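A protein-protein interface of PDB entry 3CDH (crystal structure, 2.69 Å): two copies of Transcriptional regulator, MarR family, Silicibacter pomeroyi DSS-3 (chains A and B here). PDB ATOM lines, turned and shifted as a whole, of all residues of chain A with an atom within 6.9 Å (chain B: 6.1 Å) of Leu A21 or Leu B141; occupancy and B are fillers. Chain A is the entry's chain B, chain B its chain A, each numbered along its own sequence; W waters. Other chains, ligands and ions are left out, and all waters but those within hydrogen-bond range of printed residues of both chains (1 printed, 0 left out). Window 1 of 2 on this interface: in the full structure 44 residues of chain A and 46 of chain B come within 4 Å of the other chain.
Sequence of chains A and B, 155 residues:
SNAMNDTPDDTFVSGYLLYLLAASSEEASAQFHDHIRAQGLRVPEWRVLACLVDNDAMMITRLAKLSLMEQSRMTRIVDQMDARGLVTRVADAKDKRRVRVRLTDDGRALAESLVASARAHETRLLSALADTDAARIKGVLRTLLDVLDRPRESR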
ATOM      1  N   TYR A  16      20.035  11.441   2.065  1.00  0.00           N
ATOM      2  CA  TYR A  16      20.557  12.790   2.166  1.00  0.00           C
ATOM      3  C   TYR A  16      20.293  13.372   3.551  1.00  0.00           C
ATOM      4  O   TYR A  16      19.165  13.309   4.043  1.00  0.00           O
ATOM      5  CB  TYR A  16      19.861  13.604   1.110  1.00  0.00           C
ATOM      6  CG  TYR A  16      20.186  15.052   1.028  1.00  0.00           C
ATOM      7  CD1 TYR A  16      21.485  15.522   1.193  1.00  0.00           C
ATOM      8  CD2 TYR A  16      19.181  15.969   0.724  1.00  0.00           C
ATOM      9  CE1 TYR A  16      21.771  16.886   1.087  1.00  0.00           C
ATOM     10  CE2 TYR A  16      19.456  17.317   0.609  1.00  0.00           C
ATOM     11  CZ  TYR A  16      20.746  17.766   0.787  1.00  0.00           C
ATOM     12  OH  TYR A  16      20.992  19.095   0.649  1.00  0.00           O
ATOM     13  N   LEU A  17      21.327  13.945   4.181  1.00  0.00           N
ATOM     14  CA  LEU A  17      21.199  14.429   5.554  1.00  0.00           C
ATOM     15  C   LEU A  17      20.036  15.401   5.737  1.00  0.00           C
ATOM     16  O   LEU A  17      19.275  15.277   6.700  1.00  0.00           O
ATOM     17  CB  LEU A  17      22.483  15.060   6.064  1.00  0.00           C
ATOM     18  CG  LEU A  17      22.311  15.598   7.508  1.00  0.00           C
ATOM     19  CD1 LEU A  17      22.096  14.501   8.539  1.00  0.00           C
ATOM     20  CD2 LEU A  17      23.463  16.507   7.951  1.00  0.00           C
ATOM     21  N   LEU A  18      19.903  16.352   4.811  1.00  0.00           N
ATOM     22  CA  LEU A  18      18.887  17.400   4.910  1.00  0.00           C
ATOM     23  C   LEU A  18      17.476  16.832   4.772  1.00  0.00           C
ATOM     24  O   LEU A  18      16.546  17.261   5.468  1.00  0.00           O
ATOM     25  CB  LEU A  18      19.155  18.528   3.914  1.00  0.00           C
ATOM     26  CG  LEU A  18      19.981  19.710   4.468  1.00  0.00           C
ATOM     27  CD1 LEU A  18      21.103  19.280   5.388  1.00  0.00           C
ATOM     28  CD2 LEU A  18      20.546  20.563   3.359  1.00  0.00           C
ATOM     29  N   TYR A  19      17.331  15.823   3.915  1.00  0.00           N
ATOM     30  CA  TYR A  19      16.068  15.126   3.812  1.00  0.00           C
ATOM     31  C   TYR A  19      15.762  14.416   5.127  1.00  0.00           C
ATOM     32  O   TYR A  19      14.671  14.563   5.680  1.00  0.00           O
ATOM     33  CB  TYR A  19      16.052  14.144   2.646  1.00  0.00           C
ATOM     34  CG  TYR A  19      14.873  13.220   2.742  1.00  0.00           C
ATOM     35  CD1 TYR A  19      15.010  11.951   3.300  1.00  0.00           C
ATOM     36  CD2 TYR A  19      13.600  13.627   2.345  1.00  0.00           C
ATOM     37  CE1 TYR A  19      13.926  11.094   3.422  1.00  0.00           C
ATOM     38  CE2 TYR A  19      12.513  12.776   2.450  1.00  0.00           C
ATOM     39  CZ  TYR A  19      12.692  11.523   2.998  1.00  0.00           C
ATOM     40  OH  TYR A  19      11.651  10.674   3.115  1.00  0.00           O
ATOM     41  N   LEU A  20      16.729  13.657   5.637  1.00  0.00           N
ATOM     42  CA  LEU A  20      16.519  12.912   6.859  1.00  0.00           C
ATOM     43  C   LEU A  20      16.183  13.854   8.002  1.00  0.00           C
ATOM     44  O   LEU A  20      15.296  13.549   8.802  1.00  0.00           O
ATOM     45  CB  LEU A  20      17.730  12.087   7.197  1.00  0.00           C
ATOM     46  CG  LEU A  20      17.977  10.924   6.241  1.00  0.00           C
ATOM     47  CD1 LEU A  20      19.359  10.384   6.511  1.00  0.00           C
ATOM     48  CD2 LEU A  20      16.937   9.839   6.350  1.00  0.00           C
ATOM     49  N   LEU A  21      16.850  15.008   8.086  1.00  0.00           N
ATOM     50  CA  LEU A  21      16.493  15.952   9.146  1.00  0.00           C
ATOM     51  C   LEU A  21      15.048  16.449   8.975  1.00  0.00           C
ATOM     52  O   LEU A  21      14.242  16.396   9.917  1.00  0.00           O
ATOM     53  CB  LEU A  21      17.470  17.120   9.195  1.00  0.00           C
ATOM     54  CG  LEU A  21      18.832  16.891   9.872  1.00  0.00           C
ATOM     55  CD1 LEU A  21      19.753  18.078   9.659  1.00  0.00           C
ATOM     56  CD2 LEU A  21      18.701  16.601  11.356  1.00  0.00           C
ATOM     57  N   ALA A  22      14.712  16.889   7.761  1.00  0.00           N
ATOM     58  CA  ALA A  22      13.433  17.538   7.541  1.00  0.00           C
ATOM     59  C   ALA A  22      12.258  16.565   7.702  1.00  0.00           C
ATOM     60  O   ALA A  22      11.248  16.901   8.324  1.00  0.00           O
ATOM     61  CB  ALA A  22      13.413  18.209   6.206  1.00  0.00           C
ATOM     62  N   ALA A  23      12.403  15.360   7.173  1.00  0.00           N
ATOM     63  CA  ALA A  23      11.384  14.330   7.324  1.00  0.00           C
ATOM     64  C   ALA A  23      11.178  13.970   8.800  1.00  0.00           C
ATOM     65  O   ALA A  23      10.033  13.904   9.283  1.00  0.00           O
ATOM     66  CB  ALA A  23      11.748  13.101   6.521  1.00  0.00           C
ATOM     67  N   SER A  24      12.272  13.755   9.519  1.00  0.00           N
ATOM     68  CA  SER A  24      12.204  13.463  10.943  1.00  0.00           C
ATOM     69  C   SER A  24      11.420  14.508  11.699  1.00  0.00           C
ATOM     70  O   SER A  24      10.535  14.189  12.497  1.00  0.00           O
ATOM     71  CB  SER A  24      13.592  13.442  11.532  1.00  0.00           C
ATOM     72  OG  SER A  24      14.280  12.349  11.000  1.00  0.00           O
ATOM     73  N   SER A  25      11.760  15.765  11.461  1.00  0.00           N
ATOM     74  CA  SER A  25      11.169  16.820  12.231  1.00  0.00           C
ATOM     75  C   SER A  25       9.656  16.824  11.919  1.00  0.00           C
ATOM     76  O   SER A  25       8.829  16.935  12.820  1.00  0.00           O
ATOM     77  CB  SER A  25      11.851  18.135  11.880  1.00  0.00           C
ATOM     78  OG  SER A  25      11.209  19.221  12.505  1.00  0.00           O
ATOM     79  N   GLU A  26       9.309  16.657  10.647  1.00  0.00           N
ATOM     80  CA  GLU A  26       7.939  16.587  10.245  1.00  0.00           C
ATOM     81  C   GLU A  26       7.200  15.419  10.916  1.00  0.00           C
ATOM     82  O   GLU A  26       6.156  15.612  11.558  1.00  0.00           O
ATOM     83  CB  GLU A  26       7.919  16.385   8.763  1.00  0.00           C
ATOM     84  CG  GLU A  26       6.589  15.973   8.198  1.00  0.00           C
ATOM     85  CD  GLU A  26       6.074  17.027   7.267  1.00  0.00           C
ATOM     86  OE1 GLU A  26       6.135  18.221   7.668  1.00  0.00           O
ATOM     87  OE2 GLU A  26       5.649  16.660   6.131  1.00  0.00           O
ATOM     88  N   ALA A 134      18.630   5.320  18.133  1.00  0.00           N
ATOM     89  CA  ALA A 134      18.204   6.689  18.346  1.00  0.00           C
ATOM     90  C   ALA A 134      18.057   7.077  19.827  1.00  0.00           C
ATOM     91  O   ALA A 134      17.641   8.181  20.139  1.00  0.00           O
ATOM     92  CB  ALA A 134      16.905   6.939  17.581  1.00  0.00           C
ATOM     93  N   ILE A 137      19.176  10.549  20.646  1.00  0.00           N
ATOM     94  CA  ILE A 137      18.792  11.559  19.652  1.00  0.00           C
ATOM     95  C   ILE A 137      18.983  12.997  20.163  1.00  0.00           C
ATOM     96  O   ILE A 137      19.450  13.868  19.444  1.00  0.00           O
ATOM     97  CB  ILE A 137      17.331  11.331  19.129  1.00  0.00           C
ATOM     98  CG1 ILE A 137      16.869  12.442  18.188  1.00  0.00           C
ATOM     99  CG2 ILE A 137      16.325  11.299  20.252  1.00  0.00           C
ATOM    100  CD1 ILE A 137      17.353  12.330  16.771  1.00  0.00           C
ATOM    101  N   VAL A 140      22.607  14.030  20.372  1.00  0.00           N
ATOM    102  CA  VAL A 140      23.071  14.043  19.018  1.00  0.00           C
ATOM    103  C   VAL A 140      22.730  15.385  18.390  1.00  0.00           C
ATOM    104  O   VAL A 140      23.612  16.042  17.811  1.00  0.00           O
ATOM    105  CB  VAL A 140      22.456  12.873  18.230  1.00  0.00           C
ATOM    106  CG1 VAL A 140      22.665  13.035  16.721  1.00  0.00           C
ATOM    107  CG2 VAL A 140      23.049  11.553  18.714  1.00  0.00           C
ATOM    108  N   LEU A 141      21.468  15.803  18.539  1.00  0.00           N
ATOM    109  CA  LEU A 141      20.975  17.024  17.898  1.00  0.00           C
ATOM    110  C   LEU A 141      21.606  18.251  18.542  1.00  0.00           C
ATOM    111  O   LEU A 141      22.004  19.195  17.846  1.00  0.00           O
ATOM    112  CB  LEU A 141      19.440  17.082  17.908  1.00  0.00           C
ATOM    113  CG  LEU A 141      18.672  15.960  17.205  1.00  0.00           C
ATOM    114  CD1 LEU A 141      17.197  16.065  17.522  1.00  0.00           C
ATOM    115  CD2 LEU A 141      18.900  15.982  15.708  1.00  0.00           C
ATOM    116  N   LEU A 144      24.829  18.555  17.061  1.00  0.00           N
ATOM    117  CA  LEU A 144      24.681  19.085  15.719  1.00  0.00           C
ATOM    118  C   LEU A 144      24.557  20.616  15.718  1.00  0.00           C
ATOM    119  O   LEU A 144      25.319  21.308  15.004  1.00  0.00           O
ATOM    120  CB  LEU A 144      23.516  18.418  14.986  1.00  0.00           C
ATOM    121  CG  LEU A 144      23.072  19.028  13.653  1.00  0.00           C
ATOM    122  CD1 LEU A 144      24.207  19.108  12.635  1.00  0.00           C
ATOM    123  CD2 LEU A 144      21.896  18.246  13.095  1.00  0.00           C
ATOM    124  N   LEU A 148      26.832  23.538  14.204  1.00  0.00           N
ATOM    125  CA  LEU A 148      26.255  24.378  13.162  1.00  0.00           C
ATOM    126  C   LEU A 148      26.406  25.857  13.500  1.00  0.00           C
ATOM    127  O   LEU A 148      25.953  26.724  12.753  1.00  0.00           O
ATOM    128  CB  LEU A 148      24.779  24.035  12.952  1.00  0.00           C
ATOM    129  CG  LEU A 148      24.484  22.835  12.048  1.00  0.00           C
ATOM    130  CD1 LEU A 148      23.068  22.328  12.274  1.00  0.00           C
ATOM    131  CD2 LEU A 148      24.701  23.198  10.586  1.00  0.00           C
ATOM    132  N   LEU B  21      14.814  18.979  16.776  1.00  0.00           N
ATOM    133  CA  LEU B  21      14.706  18.505  15.390  1.00  0.00           C
ATOM    134  C   LEU B  21      14.466  19.657  14.430  1.00  0.00           C
ATOM    135  O   LEU B  21      15.219  19.838  13.490  1.00  0.00           O
ATOM    136  CB  LEU B  21      13.614  17.463  15.244  1.00  0.00           C
ATOM    137  CG  LEU B  21      13.987  16.079  15.743  1.00  0.00           C
ATOM    138  CD1 LEU B  21      12.742  15.297  15.945  1.00  0.00           C
ATOM    139  CD2 LEU B  21      14.901  15.369  14.756  1.00  0.00           C
ATOM    140  N   SER B  24      17.604  22.065  14.103  1.00  0.00           N
ATOM    141  CA  SER B  24      18.665  21.372  13.369  1.00  0.00           C
ATOM    142  C   SER B  24      18.398  21.418  11.888  1.00  0.00           C
ATOM    143  O   SER B  24      19.255  21.867  11.113  1.00  0.00           O
ATOM    144  CB  SER B  24      18.740  19.909  13.746  1.00  0.00           C
ATOM    145  OG  SER B  24      19.017  19.787  15.110  1.00  0.00           O
ATOM    146  N   SER B  25      17.205  20.947  11.513  1.00  0.00           N
ATOM    147  CA  SER B  25      16.804  20.858  10.138  1.00  0.00           C
ATOM    148  C   SER B  25      16.870  22.234   9.496  1.00  0.00           C
ATOM    149  O   SER B  25      17.386  22.377   8.386  1.00  0.00           O
ATOM    150  CB  SER B  25      15.406  20.266  10.058  1.00  0.00           C
ATOM    151  OG  SER B  25      14.887  20.295   8.747  1.00  0.00           O
ATOM    152  N   ALA B  28      20.642  23.387   9.309  1.00  0.00           N
ATOM    153  CA  ALA B  28      21.459  22.642   8.360  1.00  0.00           C
ATOM    154  C   ALA B  28      21.116  23.065   6.945  1.00  0.00           C
ATOM    155  O   ALA B  28      21.988  23.166   6.095  1.00  0.00           O
ATOM    156  CB  ALA B  28      21.277  21.162   8.544  1.00  0.00           C
ATOM    157  N   SER B  29      19.842  23.332   6.720  1.00  0.00           N
ATOM    158  CA  SER B  29      19.326  23.716   5.422  1.00  0.00           C
ATOM    159  C   SER B  29      19.645  25.124   5.015  1.00  0.00           C
ATOM    160  O   SER B  29      19.820  25.379   3.846  1.00  0.00           O
ATOM    161  CB  SER B  29      17.825  23.628   5.447  1.00  0.00           C
ATOM    162  OG  SER B  29      17.475  22.276   5.531  1.00  0.00           O
ATOM    163  N   LEU B 125      29.447  19.206   6.219  1.00  0.00           N
ATOM    164  CA  LEU B 125      28.750  19.073   7.506  1.00  0.00           C
ATOM    165  C   LEU B 125      29.115  17.780   8.243  1.00  0.00           C
ATOM    166  O   LEU B 125      29.452  17.803   9.457  1.00  0.00           O
ATOM    167  CB  LEU B 125      27.249  19.147   7.326  1.00  0.00           C
ATOM    168  CG  LEU B 125      26.459  20.070   8.261  1.00  0.00           C
ATOM    169  CD1 LEU B 125      24.965  19.727   8.144  1.00  0.00           C
ATOM    170  CD2 LEU B 125      26.924  20.012   9.715  1.00  0.00           C
ATOM    171  N   ARG B 136      27.266   9.513  13.908  1.00  0.00           N
ATOM    172  CA  ARG B 136      26.301   8.572  13.321  1.00  0.00           C
ATOM    173  C   ARG B 136      24.901   9.177  13.048  1.00  0.00           C
ATOM    174  O   ARG B 136      23.906   8.450  13.031  1.00  0.00           O
ATOM    175  CB  ARG B 136      26.205   7.292  14.189  1.00  0.00           C
ATOM    176  CG  ARG B 136      27.500   6.420  14.178  1.00  0.00           C
ATOM    177  CD  ARG B 136      27.437   5.118  15.022  1.00  0.00           C
ATOM    178  NE  ARG B 136      28.792   4.658  15.359  1.00  0.00           N
ATOM    179  CZ  ARG B 136      29.501   3.749  14.687  1.00  0.00           C
ATOM    180  NH1 ARG B 136      30.725   3.451  15.095  1.00  0.00           N
ATOM    181  NH2 ARG B 136      29.000   3.129  13.621  1.00  0.00           N
ATOM    182  N   ILE B 137      24.826  10.489  12.805  1.00  0.00           N
ATOM    183  CA  ILE B 137      23.538  11.173  12.729  1.00  0.00           C
ATOM    184  C   ILE B 137      22.547  10.583  11.723  1.00  0.00           C
ATOM    185  O   ILE B 137      21.371  10.355  12.056  1.00  0.00           O
ATOM    186  CB  ILE B 137      23.673  12.694  12.536  1.00  0.00           C
ATOM    187  CG1 ILE B 137      22.307  13.351  12.757  1.00  0.00           C
ATOM    188  CG2 ILE B 137      24.327  13.041  11.209  1.00  0.00           C
ATOM    189  CD1 ILE B 137      22.382  14.813  12.863  1.00  0.00           C
ATOM    190  N   LYS B 138      23.031  10.307  10.514  1.00  0.00           N
ATOM    191  CA  LYS B 138      22.211   9.645   9.526  1.00  0.00           C
ATOM    192  C   LYS B 138      21.563   8.356  10.045  1.00  0.00           C
ATOM    193  O   LYS B 138      20.358   8.168   9.915  1.00  0.00           O
ATOM    194  CB  LYS B 138      22.998   9.381   8.269  1.00  0.00           C
ATOM    195  CG  LYS B 138      23.118  10.579   7.346  1.00  0.00           C
ATOM    196  CD  LYS B 138      23.697  10.121   6.024  1.00  0.00           C
ATOM    197  CE  LYS B 138      24.078  11.308   5.228  1.00  0.00           C
ATOM    198  NZ  LYS B 138      24.343  10.929   3.823  1.00  0.00           N
ATOM    199  N   GLY B 139      22.335   7.482  10.661  1.00  0.00           N
ATOM    200  CA  GLY B 139      21.770   6.255  11.200  1.00  0.00           C
ATOM    201  C   GLY B 139      20.728   6.546  12.260  1.00  0.00           C
ATOM    202  O   GLY B 139      19.626   5.984  12.226  1.00  0.00           O
ATOM    203  N   VAL B 140      21.063   7.437  13.197  1.00  0.00           N
ATOM    204  CA  VAL B 140      20.122   7.844  14.225  1.00  0.00           C
ATOM    205  C   VAL B 140      18.785   8.264  13.622  1.00  0.00           C
ATOM    206  O   VAL B 140      17.723   7.722  14.010  1.00  0.00           O
ATOM    207  CB  VAL B 140      20.678   9.005  15.059  1.00  0.00           C
ATOM    208  CG1 VAL B 140      19.625   9.520  16.028  1.00  0.00           C
ATOM    209  CG2 VAL B 140      21.944   8.570  15.785  1.00  0.00           C
ATOM    210  N   LEU B 141      18.835   9.216  12.686  1.00  0.00           N
ATOM    211  CA  LEU B 141      17.629   9.680  12.035  1.00  0.00           C
ATOM    212  C   LEU B 141      16.873   8.540  11.328  1.00  0.00           C
ATOM    213  O   LEU B 141      15.635   8.456  11.454  1.00  0.00           O
ATOM    214  CB  LEU B 141      17.922  10.814  11.068  1.00  0.00           C
ATOM    215  CG  LEU B 141      18.548  12.039  11.706  1.00  0.00           C
ATOM    216  CD1 LEU B 141      18.940  13.091  10.680  1.00  0.00           C
ATOM    217  CD2 LEU B 141      17.623  12.637  12.731  1.00  0.00           C
ATOM    218  N   ARG B 142      17.569   7.652  10.613  1.00  0.00           N
ATOM    219  CA  ARG B 142      16.846   6.611   9.874  1.00  0.00           C
ATOM    220  C   ARG B 142      16.220   5.603  10.835  1.00  0.00           C
ATOM    221  O   ARG B 142      15.244   4.943  10.477  1.00  0.00           O
ATOM    222  CB  ARG B 142      17.714   5.904   8.826  1.00  0.00           C
ATOM    223  CG  ARG B 142      17.196   6.009   7.373  1.00  0.00           C
ATOM    224  CD  ARG B 142      16.020   5.079   6.995  1.00  0.00           C
ATOM    225  NE  ARG B 142      14.783   5.790   6.617  1.00  0.00           N
ATOM    226  CZ  ARG B 142      14.594   6.572   5.534  1.00  0.00           C
ATOM    227  NH1 ARG B 142      15.553   6.831   4.656  1.00  0.00           N
ATOM    228  NH2 ARG B 142      13.413   7.126   5.328  1.00  0.00           N
ATOM    229  N   THR B 143      16.765   5.494  12.047  1.00  0.00           N
ATOM    230  CA  THR B 143      16.140   4.697  13.076  1.00  0.00           C
ATOM    231  C   THR B 143      14.887   5.405  13.593  1.00  0.00           C
ATOM    232  O   THR B 143      13.815   4.787  13.702  1.00  0.00           O
ATOM    233  CB  THR B 143      17.106   4.471  14.242  1.00  0.00           C
ATOM    234  OG1 THR B 143      18.252   3.722  13.798  1.00  0.00           O
ATOM    235  CG2 THR B 143      16.425   3.754  15.401  1.00  0.00           C
ATOM    236  N   LEU B 144      15.015   6.698  13.907  1.00  0.00           N
ATOM    237  CA  LEU B 144      13.884   7.465  14.404  1.00  0.00           C
ATOM    238  C   LEU B 144      12.733   7.342  13.412  1.00  0.00           C
ATOM    239  O   LEU B 144      11.588   7.022  13.796  1.00  0.00           O
ATOM    240  CB  LEU B 144      14.279   8.927  14.610  1.00  0.00           C
ATOM    241  CG  LEU B 144      13.170   9.964  14.738  1.00  0.00           C
ATOM    242  CD1 LEU B 144      12.339   9.691  15.955  1.00  0.00           C
ATOM    243  CD2 LEU B 144      13.742  11.361  14.788  1.00  0.00           C
ATOM    244  N   LEU B 145      13.049   7.574  12.136  1.00  0.00           N
ATOM    245  CA  LEU B 145      12.066   7.442  11.058  1.00  0.00           C
ATOM    246  C   LEU B 145      11.421   6.053  11.011  1.00  0.00           C
ATOM    247  O   LEU B 145      10.216   5.940  10.787  1.00  0.00           O
ATOM    248  CB  LEU B 145      12.682   7.792   9.706  1.00  0.00           C
ATOM    249  CG  LEU B 145      12.843   9.274   9.386  1.00  0.00           C
ATOM    250  CD1 LEU B 145      13.533   9.385   8.071  1.00  0.00           C
ATOM    251  CD2 LEU B 145      11.512   9.989   9.319  1.00  0.00           C
ATOM    252  N   ASP B 146      12.208   5.003  11.236  1.00  0.00           N
ATOM    253  CA  ASP B 146      11.666   3.641  11.210  1.00  0.00           C
ATOM    254  C   ASP B 146      10.727   3.376  12.373  1.00  0.00           C
ATOM    255  O   ASP B 146       9.749   2.649  12.216  1.00  0.00           O
ATOM    256  CB  ASP B 146      12.781   2.584  11.206  1.00  0.00           C
ATOM    257  CG  ASP B 146      13.601   2.583   9.911  1.00  0.00           C
ATOM    258  OD1 ASP B 146      13.333   3.371   8.947  1.00  0.00           O
ATOM    259  OD2 ASP B 146      14.552   1.774   9.872  1.00  0.00           O
HETATM  260  O   HOH W   1      16.754  19.641   6.771  1.00  0.00           O
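The backbone carbonyl oxygen of Leu A20 lies within hydrogen-bond range of the side-chain hydroxyl of Ser A24, at 2.7 Å.
The guanidinium group (NE) of Arg B142 is in salt-bridge range of the side-chain carboxylate (OD1) of Asp B146.
The backbone carbonyl oxygen of Ser B25 is in hydrogen-bond range of the side-chain hydroxyl of Ser B29 (2.9 Å).
The backbone carbonyl oxygen of Gly B139 sits at hydrogen-bond distance from the side-chain hydroxyl of Thr B143 (3.1 Å).
Among the printed residues, merely in contact across the chains: Leu A17 with Leu B125 (3.6 Å), Leu A17 with Ile B137 (3.8 Å), Leu A17 with Lys B138 (3.95 Å), Leu A18 with Ala B28 (3.7 Å), Leu A18 with Ser B29 (3.7 Å), Leu A20 with Lys B138 (3.9 Å), Leu A20 with Leu B141 (3.8 Å), Leu A20 with Arg B142 (3.7 Å), Leu A20 with Leu B145 (3.8 Å), Leu A21 with Ser B25 (3.9 Å), Leu A21 with Ala B28 (3.6 Å), Leu A21 with Leu B141 (3.6 Å), Ala A22 with Ser B25 (3.3 Å), Ser A24 with Leu B21 (3.98 Å), Ser A24 with Leu B141 (3.8 Å), Ser A24 with Leu B144 (3.9 Å), Ser A24 with Leu B145 (3.8 Å), Ser A25 with Leu B21 (3.8 Å), Ala A134 with Val B140 (3.7 Å), Ala A134 with Thr B143 (3.8 Å), Ile A137 with Val B140 (3.7 Å), Val A140 with Ile B137 (3.99 Å), Leu A141 with Leu B21 (3.7 Å), Leu A141 with Ser B24 (3.9 Å), Leu A144 with Ser B24 (3.6 Å), Leu A144 with Ile B137 (3.5 Å), Leu A148 with Ala B28 (3.97 Å) and Leu A148 with Leu B125 (3.98 Å).
Tyr A19 touches none of the printed residues of chain B.
Printed residues of chain B within 4 Å of Ser A25: Leu B21.
Glu A26 touches none of the printed residues of chain B.
Of the printed residues of chain B, Leu A144 touches Ser B24 (3.6 Å) and Ile B137 (3.5 Å).
Of the printed residues of chain A, Ser B25 touches Leu A21 and Ala A22.
Printed residues of chain A within 4 Å of Ala B28: Leu A18, Leu A21 and Leu A148.
Printed residues of chain A within 4 Å of Lys B138: Leu A17 and Leu A20.
Of chain A, only Leu A20, Leu A21 and Ser A24 come within 4 Å of Leu B141.
The nearest residue of chain B that does not touch Leu A21 is Ser B24 (4.1 Å).
The nearest printed residue of chain A that does not touch Leu B141 is Ile A137 (4.1 Å).
Of the 17 printed residues of chain A, 13 touch a printed residue of chain B.
Printed residues of chain A that touch a printed residue of chain B: Leu A17, Leu A18, Leu A20, Leu A21, Ala A22, Ser A24, Ser A25, Ala A134, Ile A137, Val A140, Leu A141, Leu A144 and Leu A148.
Hydrophobic or aromatic side chains of chain A within 4 Å of the printed part of chain B: Leu A17, Leu A18, Leu A20, Leu A21, Ala A22, Ala A134, Ile A137, Val A140, Leu A141, Leu A144 and Leu A148.
Of the 17 printed residues of chain B, 14 touch a printed residue of chain A.
Hydrophobic or aromatic side chains of chain B within 4 Å of the printed part of chain A: Leu B21, Ala B28, Leu B125, Ile B137, Val B140, Leu B141, Leu B144 and Leu B145.
Along chain B the printed residues that touch a printed residue of chain A span positions 21 to 145.
Among the printed residues, 28 pairs touch across the chains.
Leu A21 touches Leu B141, and with the chains exchanged Leu A141 touches Leu B21.
Ser A24 touches Leu B21, but with the chains exchanged Leu A21 does not touch Ser B24 (4.1 Å).
Ser A24 touches Leu B141, and with the chains exchanged Leu A141 touches Ser B24.
Ser A24 touches Leu B144, and with the chains exchanged Leu A144 touches Ser B24.
Positions printed for both chains: 21, 24, 25, 137, 140, 141 and 144.
Water W1 lies within hydrogen-bond range of O of Leu A18 (2.7 Å), OG of Ser B25 (2.8 Å) and OG of Ser B29 (3.0 Å).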
